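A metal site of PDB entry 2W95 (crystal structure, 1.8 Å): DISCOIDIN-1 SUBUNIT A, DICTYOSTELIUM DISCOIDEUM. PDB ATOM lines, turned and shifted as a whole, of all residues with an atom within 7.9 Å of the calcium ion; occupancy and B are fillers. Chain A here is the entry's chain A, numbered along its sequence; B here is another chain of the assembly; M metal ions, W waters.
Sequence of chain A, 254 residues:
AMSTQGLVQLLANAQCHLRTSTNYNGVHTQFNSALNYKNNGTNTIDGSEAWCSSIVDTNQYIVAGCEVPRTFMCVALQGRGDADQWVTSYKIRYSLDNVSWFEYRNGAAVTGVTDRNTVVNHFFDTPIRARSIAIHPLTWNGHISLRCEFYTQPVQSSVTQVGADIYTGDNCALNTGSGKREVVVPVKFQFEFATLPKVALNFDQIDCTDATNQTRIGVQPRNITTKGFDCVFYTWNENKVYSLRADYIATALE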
ATOM      1  N   GLY A 163      10.532  11.353 -20.383  1.00  0.00           N
ATOM      2  CA  GLY A 163      10.854  12.575 -19.631  1.00  0.00           C
ATOM      3  C   GLY A 163      12.365  12.717 -19.475  1.00  0.00           C
ATOM      4  O   GLY A 163      13.093  11.726 -19.371  1.00  0.00           O
ATOM      5  N   ALA A 164      12.861  13.946 -19.546  1.00  0.00           N
ATOM      6  CA  ALA A 164      14.292  14.145 -19.609  1.00  0.00           C
ATOM      7  C   ALA A 164      14.810  14.864 -18.347  1.00  0.00           C
ATOM      8  O   ALA A 164      14.102  15.691 -17.760  1.00  0.00           O
ATOM      9  CB  ALA A 164      14.656  14.964 -20.840  1.00  0.00           C
ATOM     10  N   ASP A 165      16.036  14.514 -17.986  1.00  0.00           N
ATOM     11  CA  ASP A 165      16.909  15.368 -17.161  1.00  0.00           C
ATOM     12  C   ASP A 165      16.454  15.472 -15.712  1.00  0.00           C
ATOM     13  O   ASP A 165      16.420  16.549 -15.128  1.00  0.00           O
ATOM     14  CB  ASP A 165      17.055  16.756 -17.787  1.00  0.00           C
ATOM     15  CG  ASP A 165      17.528  16.681 -19.236  1.00  0.00           C
ATOM     16  OD1 ASP A 165      18.142  15.665 -19.665  1.00  0.00           O
ATOM     17  OD2 ASP A 165      17.222  17.619 -19.964  1.00  0.00           O
ATOM     18  N   ILE A 166      16.063  14.328 -15.154  1.00  0.00           N
ATOM     19  CA  ILE A 166      15.799  14.222 -13.756  1.00  0.00           C
ATOM     20  C   ILE A 166      17.183  14.288 -13.068  1.00  0.00           C
ATOM     21  O   ILE A 166      18.029  13.517 -13.431  1.00  0.00           O
ATOM     22  CB  ILE A 166      15.132  12.901 -13.409  1.00  0.00           C
ATOM     23  CG1 ILE A 166      13.933  12.578 -14.340  1.00  0.00           C
ATOM     24  CG2 ILE A 166      14.699  12.866 -11.990  1.00  0.00           C
ATOM     25  CD1 ILE A 166      13.018  13.721 -14.636  1.00  0.00           C
ATOM     26  N   ASN A 202      17.624   5.709 -16.797  1.00  0.00           N
ATOM     27  CA  ASN A 202      19.016   5.415 -17.123  1.00  0.00           C
ATOM     28  C   ASN A 202      19.835   6.696 -17.119  1.00  0.00           C
ATOM     29  O   ASN A 202      19.290   7.793 -17.148  1.00  0.00           O
ATOM     30  CB  ASN A 202      19.145   4.758 -18.496  1.00  0.00           C
ATOM     31  CG  ASN A 202      18.354   3.483 -18.608  1.00  0.00           C
ATOM     32  OD1 ASN A 202      17.515   3.351 -19.492  1.00  0.00           O
ATOM     33  ND2 ASN A 202      18.616   2.527 -17.724  1.00  0.00           N
ATOM     34  N   PHE A 203      21.158   6.546 -16.946  1.00  0.00           N
ATOM     35  CA  PHE A 203      22.013   7.716 -16.788  1.00  0.00           C
ATOM     36  C   PHE A 203      22.258   8.472 -18.075  1.00  0.00           C
ATOM     37  O   PHE A 203      22.488   7.863 -19.122  1.00  0.00           O
ATOM     38  CB  PHE A 203      23.389   7.270 -16.270  1.00  0.00           C
ATOM     39  CG  PHE A 203      23.361   6.667 -14.902  1.00  0.00           C
ATOM     40  CD1 PHE A 203      23.776   5.362 -14.705  1.00  0.00           C
ATOM     41  CD2 PHE A 203      22.978   7.418 -13.825  1.00  0.00           C
ATOM     42  CE1 PHE A 203      23.778   4.825 -13.447  1.00  0.00           C
ATOM     43  CE2 PHE A 203      23.008   6.884 -12.576  1.00  0.00           C
ATOM     44  CZ  PHE A 203      23.389   5.572 -12.400  1.00  0.00           C
ATOM     45  N   ASP A 204      22.311   9.808 -17.977  1.00  0.00           N
ATOM     46  CA  ASP A 204      22.846  10.638 -19.043  1.00  0.00           C
ATOM     47  C   ASP A 204      23.953  11.595 -18.545  1.00  0.00           C
ATOM     48  O   ASP A 204      24.641  12.186 -19.373  1.00  0.00           O
ATOM     49  CB  ASP A 204      21.779  11.443 -19.780  1.00  0.00           C
ATOM     50  CG  ASP A 204      21.141  12.485 -18.948  1.00  0.00           C
ATOM     51  OD1 ASP A 204      21.166  12.395 -17.700  1.00  0.00           O
ATOM     52  OD2 ASP A 204      20.604  13.487 -19.490  1.00  0.00           O
ATOM     53  N   GLN A 205      24.133  11.761 -17.226  1.00  0.00           N
ATOM     54  CA  GLN A 205      25.279  12.590 -16.769  1.00  0.00           C
ATOM     55  C   GLN A 205      25.798  12.025 -15.438  1.00  0.00           C
ATOM     56  O   GLN A 205      25.011  11.785 -14.522  1.00  0.00           O
ATOM     57  CB  GLN A 205      24.926  14.067 -16.614  1.00  0.00           C
ATOM     58  CG  GLN A 205      26.145  14.999 -16.451  1.00  0.00           C
ATOM     59  CD  GLN A 205      25.748  16.428 -16.244  1.00  0.00           C
ATOM     60  OE1 GLN A 205      25.678  17.232 -17.183  1.00  0.00           O
ATOM     61  NE2 GLN A 205      25.446  16.754 -15.006  1.00  0.00           N
ATOM     62  N   ARG A 245      22.425  12.408 -13.304  1.00  0.00           N
ATOM     63  CA  ARG A 245      21.248  12.784 -14.090  1.00  0.00           C
ATOM     64  C   ARG A 245      20.762  11.578 -14.888  1.00  0.00           C
ATOM     65  O   ARG A 245      21.538  10.695 -15.275  1.00  0.00           O
ATOM     66  CB  ARG A 245      21.535  13.962 -15.016  1.00  0.00           C
ATOM     67  CG  ARG A 245      20.328  14.769 -15.384  1.00  0.00           C
ATOM     68  CD  ARG A 245      20.660  16.000 -16.246  1.00  0.00           C
ATOM     69  NE  ARG A 245      21.238  15.561 -17.514  1.00  0.00           N
ATOM     70  CZ  ARG A 245      22.192  16.194 -18.187  1.00  0.00           C
ATOM     71  NH1 ARG A 245      22.735  17.312 -17.711  1.00  0.00           N
ATOM     72  NH2 ARG A 245      22.621  15.665 -19.316  1.00  0.00           N
ATOM     73  N   ALA A 246      19.438  11.529 -15.112  1.00  0.00           N
ATOM     74  CA  ALA A 246      18.823  10.376 -15.794  1.00  0.00           C
ATOM     75  C   ALA A 246      17.654  10.855 -16.666  1.00  0.00           C
ATOM     76  O   ALA A 246      17.050  11.868 -16.372  1.00  0.00           O
ATOM     77  CB  ALA A 246      18.325   9.365 -14.787  1.00  0.00           C
ATOM     78  N   ASP A 247      17.396  10.123 -17.746  1.00  0.00           N
ATOM     79  CA  ASP A 247      16.135  10.280 -18.497  1.00  0.00           C
ATOM     80  C   ASP A 247      15.262   9.041 -18.266  1.00  0.00           C
ATOM     81  O   ASP A 247      15.797   7.957 -17.910  1.00  0.00           O
ATOM     82  CB  ASP A 247      16.377  10.461 -20.001  1.00  0.00           C
ATOM     83  CG  ASP A 247      17.344  11.575 -20.345  1.00  0.00           C
ATOM     84  OD1 ASP A 247      17.285  12.626 -19.750  1.00  0.00           O
ATOM     85  OD2 ASP A 247      18.085  11.363 -21.329  1.00  0.00           O
ATOM     86  N   TYR A 248      13.940   9.188 -18.402  1.00  0.00           N
ATOM     87  CA  TYR A 248      13.047   8.055 -18.233  1.00  0.00           C
ATOM     88  C   TYR A 248      12.182   7.798 -19.464  1.00  0.00           C
ATOM     89  O   TYR A 248      11.892   8.714 -20.272  1.00  0.00           O
ATOM     90  CB  TYR A 248      12.173   8.146 -17.008  1.00  0.00           C
ATOM     91  CG  TYR A 248      11.029   9.097 -17.075  1.00  0.00           C
ATOM     92  CD1 TYR A 248      11.165  10.378 -16.605  1.00  0.00           C
ATOM     93  CD2 TYR A 248       9.789   8.717 -17.584  1.00  0.00           C
ATOM     94  CE1 TYR A 248      10.138  11.255 -16.645  1.00  0.00           C
ATOM     95  CE2 TYR A 248       8.746   9.597 -17.618  1.00  0.00           C
ATOM     96  CZ  TYR A 248       8.926  10.866 -17.158  1.00  0.00           C
ATOM     97  OH  TYR A 248       7.884  11.756 -17.159  1.00  0.00           O
ATOM     98  N   VAL B 199      13.126  13.449 -26.099  1.00  0.00           N
ATOM     99  CA  VAL B 199      14.205  12.514 -26.342  1.00  0.00           C
ATOM    100  C   VAL B 199      14.949  12.120 -25.065  1.00  0.00           C
ATOM    101  O   VAL B 199      15.442  12.995 -24.326  1.00  0.00           O
ATOM    102  CB  VAL B 199      15.213  13.056 -27.391  1.00  0.00           C
ATOM    103  CG1 VAL B 199      16.333  12.025 -27.669  1.00  0.00           C
ATOM    104  CG2 VAL B 199      14.489  13.425 -28.671  1.00  0.00           C
ATOM    105  N   ALA B 200      14.977  10.818 -24.818  1.00  0.00           N
ATOM    106  CA  ALA B 200      15.851  10.173 -23.833  1.00  0.00           C
ATOM    107  C   ALA B 200      17.122   9.709 -24.552  1.00  0.00           C
ATOM    108  O   ALA B 200      17.057   9.085 -25.614  1.00  0.00           O
ATOM    109  CB  ALA B 200      15.175   9.024 -23.154  1.00  0.00           C
ATOM    110  N   LEU B 201      18.294  10.034 -23.970  1.00  0.00           N
ATOM    111  CA  LEU B 201      19.557   9.734 -24.612  1.00  0.00           C
ATOM    112  C   LEU B 201      20.547   9.326 -23.486  1.00  0.00           C
ATOM    113  O   LEU B 201      20.904  10.159 -22.662  1.00  0.00           O
ATOM    114  CB  LEU B 201      20.023  10.959 -25.399  1.00  0.00           C
ATOM    115  CG  LEU B 201      21.354  10.968 -26.119  1.00  0.00           C
ATOM    116  CD1 LEU B 201      21.410   9.961 -27.215  1.00  0.00           C
ATOM    117  CD2 LEU B 201      21.600  12.436 -26.601  1.00  0.00           C
ATOM    118  N   ASN B 202      20.850   8.042 -23.444  1.00  0.00           N
ATOM    119  CA  ASN B 202      21.490   7.397 -22.286  1.00  0.00           C
ATOM    120  C   ASN B 202      22.657   6.460 -22.675  1.00  0.00           C
ATOM    121  O   ASN B 202      22.714   5.940 -23.818  1.00  0.00           O
ATOM    122  CB  ASN B 202      20.423   6.646 -21.484  1.00  0.00           C
ATOM    123  CG  ASN B 202      19.270   7.515 -21.115  1.00  0.00           C
ATOM    124  OD1 ASN B 202      18.124   7.218 -21.493  1.00  0.00           O
ATOM    125  ND2 ASN B 202      19.533   8.578 -20.370  1.00  0.00           N
ATOM    126  N   VAL B 219      25.871  13.145 -21.814  1.00  0.00           N
ATOM    127  CA  VAL B 219      25.375  13.116 -23.185  1.00  0.00           C
ATOM    128  C   VAL B 219      23.987  13.747 -23.153  1.00  0.00           C
ATOM    129  O   VAL B 219      23.234  13.519 -22.200  1.00  0.00           O
ATOM    130  CB  VAL B 219      25.316  11.699 -23.757  1.00  0.00           C
ATOM    131  CG1 VAL B 219      24.412  10.800 -22.960  1.00  0.00           C
ATOM    132  CG2 VAL B 219      24.906  11.763 -25.221  1.00  0.00           C
ATOM    133  N   GLN B 220      23.674  14.626 -24.105  1.00  0.00           N
ATOM    134  CA  GLN B 220      22.421  15.352 -24.054  1.00  0.00           C
ATOM    135  C   GLN B 220      22.026  15.747 -25.497  1.00  0.00           C
ATOM    136  O   GLN B 220      22.903  16.100 -26.305  1.00  0.00           O
ATOM    137  CB  GLN B 220      22.621  16.609 -23.191  1.00  0.00           C
ATOM    138  CG  GLN B 220      21.428  17.498 -23.018  1.00  0.00           C
ATOM    139  CD  GLN B 220      20.316  16.912 -22.156  1.00  0.00           C
ATOM    140  OE1 GLN B 220      20.298  15.722 -21.830  1.00  0.00           O
ATOM    141  NE2 GLN B 220      19.353  17.764 -21.804  1.00  0.00           N
ATOM    142  N   PRO B 221      20.715  15.705 -25.823  1.00  0.00           N
ATOM    143  CA  PRO B 221      20.261  16.225 -27.111  1.00  0.00           C
ATOM    144  C   PRO B 221      20.231  17.737 -27.090  1.00  0.00           C
ATOM    145  O   PRO B 221      19.992  18.357 -26.053  1.00  0.00           O
ATOM    146  CB  PRO B 221      18.830  15.648 -27.237  1.00  0.00           C
ATOM    147  CG  PRO B 221      18.628  14.757 -26.093  1.00  0.00           C
ATOM    148  CD  PRO B 221      19.598  15.164 -25.026  1.00  0.00           C
ATOM    149  N   TYR B 234      29.910  15.072 -23.933  1.00  0.00           N
ATOM    150  CA  TYR B 234      30.749  16.064 -23.334  1.00  0.00           C
ATOM    151  C   TYR B 234      31.440  15.574 -22.076  1.00  0.00           C
ATOM    152  O   TYR B 234      31.058  14.596 -21.432  1.00  0.00           O
ATOM    153  CB  TYR B 234      29.970  17.352 -23.057  1.00  0.00           C
ATOM    154  CG  TYR B 234      28.742  17.173 -22.158  1.00  0.00           C
ATOM    155  CD1 TYR B 234      28.823  17.382 -20.787  1.00  0.00           C
ATOM    156  CD2 TYR B 234      27.517  16.758 -22.679  1.00  0.00           C
ATOM    157  CE1 TYR B 234      27.704  17.228 -19.958  1.00  0.00           C
ATOM    158  CE2 TYR B 234      26.416  16.561 -21.866  1.00  0.00           C
ATOM    159  CZ  TYR B 234      26.502  16.794 -20.492  1.00  0.00           C
ATOM    160  OH  TYR B 234      25.387  16.658 -19.676  1.00  0.00           O
HETATM  161 CA    CA M   1      18.909  13.904 -21.043  1.00  0.00          CA
HETATM  162  O   HOH W   1      17.411  14.338 -22.889  1.00  0.00           O
HETATM  163  O   HOH W   2      20.534  12.820 -22.479  1.00  0.00           O
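The calcium ion is bound by OD2 of Asp 204 (2.3 Å), OD1 of Asp 165 (2.4 Å), water W1 (2.4 Å), OE1 of Gln 220 of chain B (2.4 Å), water W2 (2.4 Å), OD1 of Asp 247 (2.4 Å) and OD2 of Asp 247 (2.7 Å).
The calcium ion has seven donor atoms within binding distance.
The backbone NH (N) of Ala 246 is in hydrogen-bond range of the side-chain carboxylate (OD1) of Asp 204 (3.2 Å).
The side-chain amide nitrogen (ND2) of Asn 202 of chain B lies close to the side-chain carboxylate (OD2) of Asp 247 (3.3 Å).
The backbone NH (N) of Asp 165 sits at hydrogen-bond distance from the backbone carbonyl oxygen (O) of Ala 246 (3.3 Å).
The backbone NH (N) of Leu 201 of chain B lies close to the side-chain carboxylate (OD2) of Asp 247.
OE1 of Gln 220 of chain B lies close to NH2 of Arg 245, 3.4 Å away.
The backbone carbonyl oxygen (O) of Asp 204 is in hydrogen-bond range of the backbone NH (N) of Val 219 of chain B (2.9 Å).
O of Asn 202 of chain A sits at hydrogen-bond distance from N of Asp 247 (3.1 Å).
The side-chain carboxylate (OD1) of Asp 165 lies close to the guanidinium group (NE) of Arg 245 (3.8 Å).
Four residues have an atom within 4 Å of the calcium ion: Asp 165, Asp 204, Asp 247 and Gln 220 of chain B.
Water W2 bridges the backbone carbonyl oxygen (O) of Leu 201 of chain B (2.7 Å) and the backbone carbonyl oxygen (O) of Val 219 of chain B (2.8 Å).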
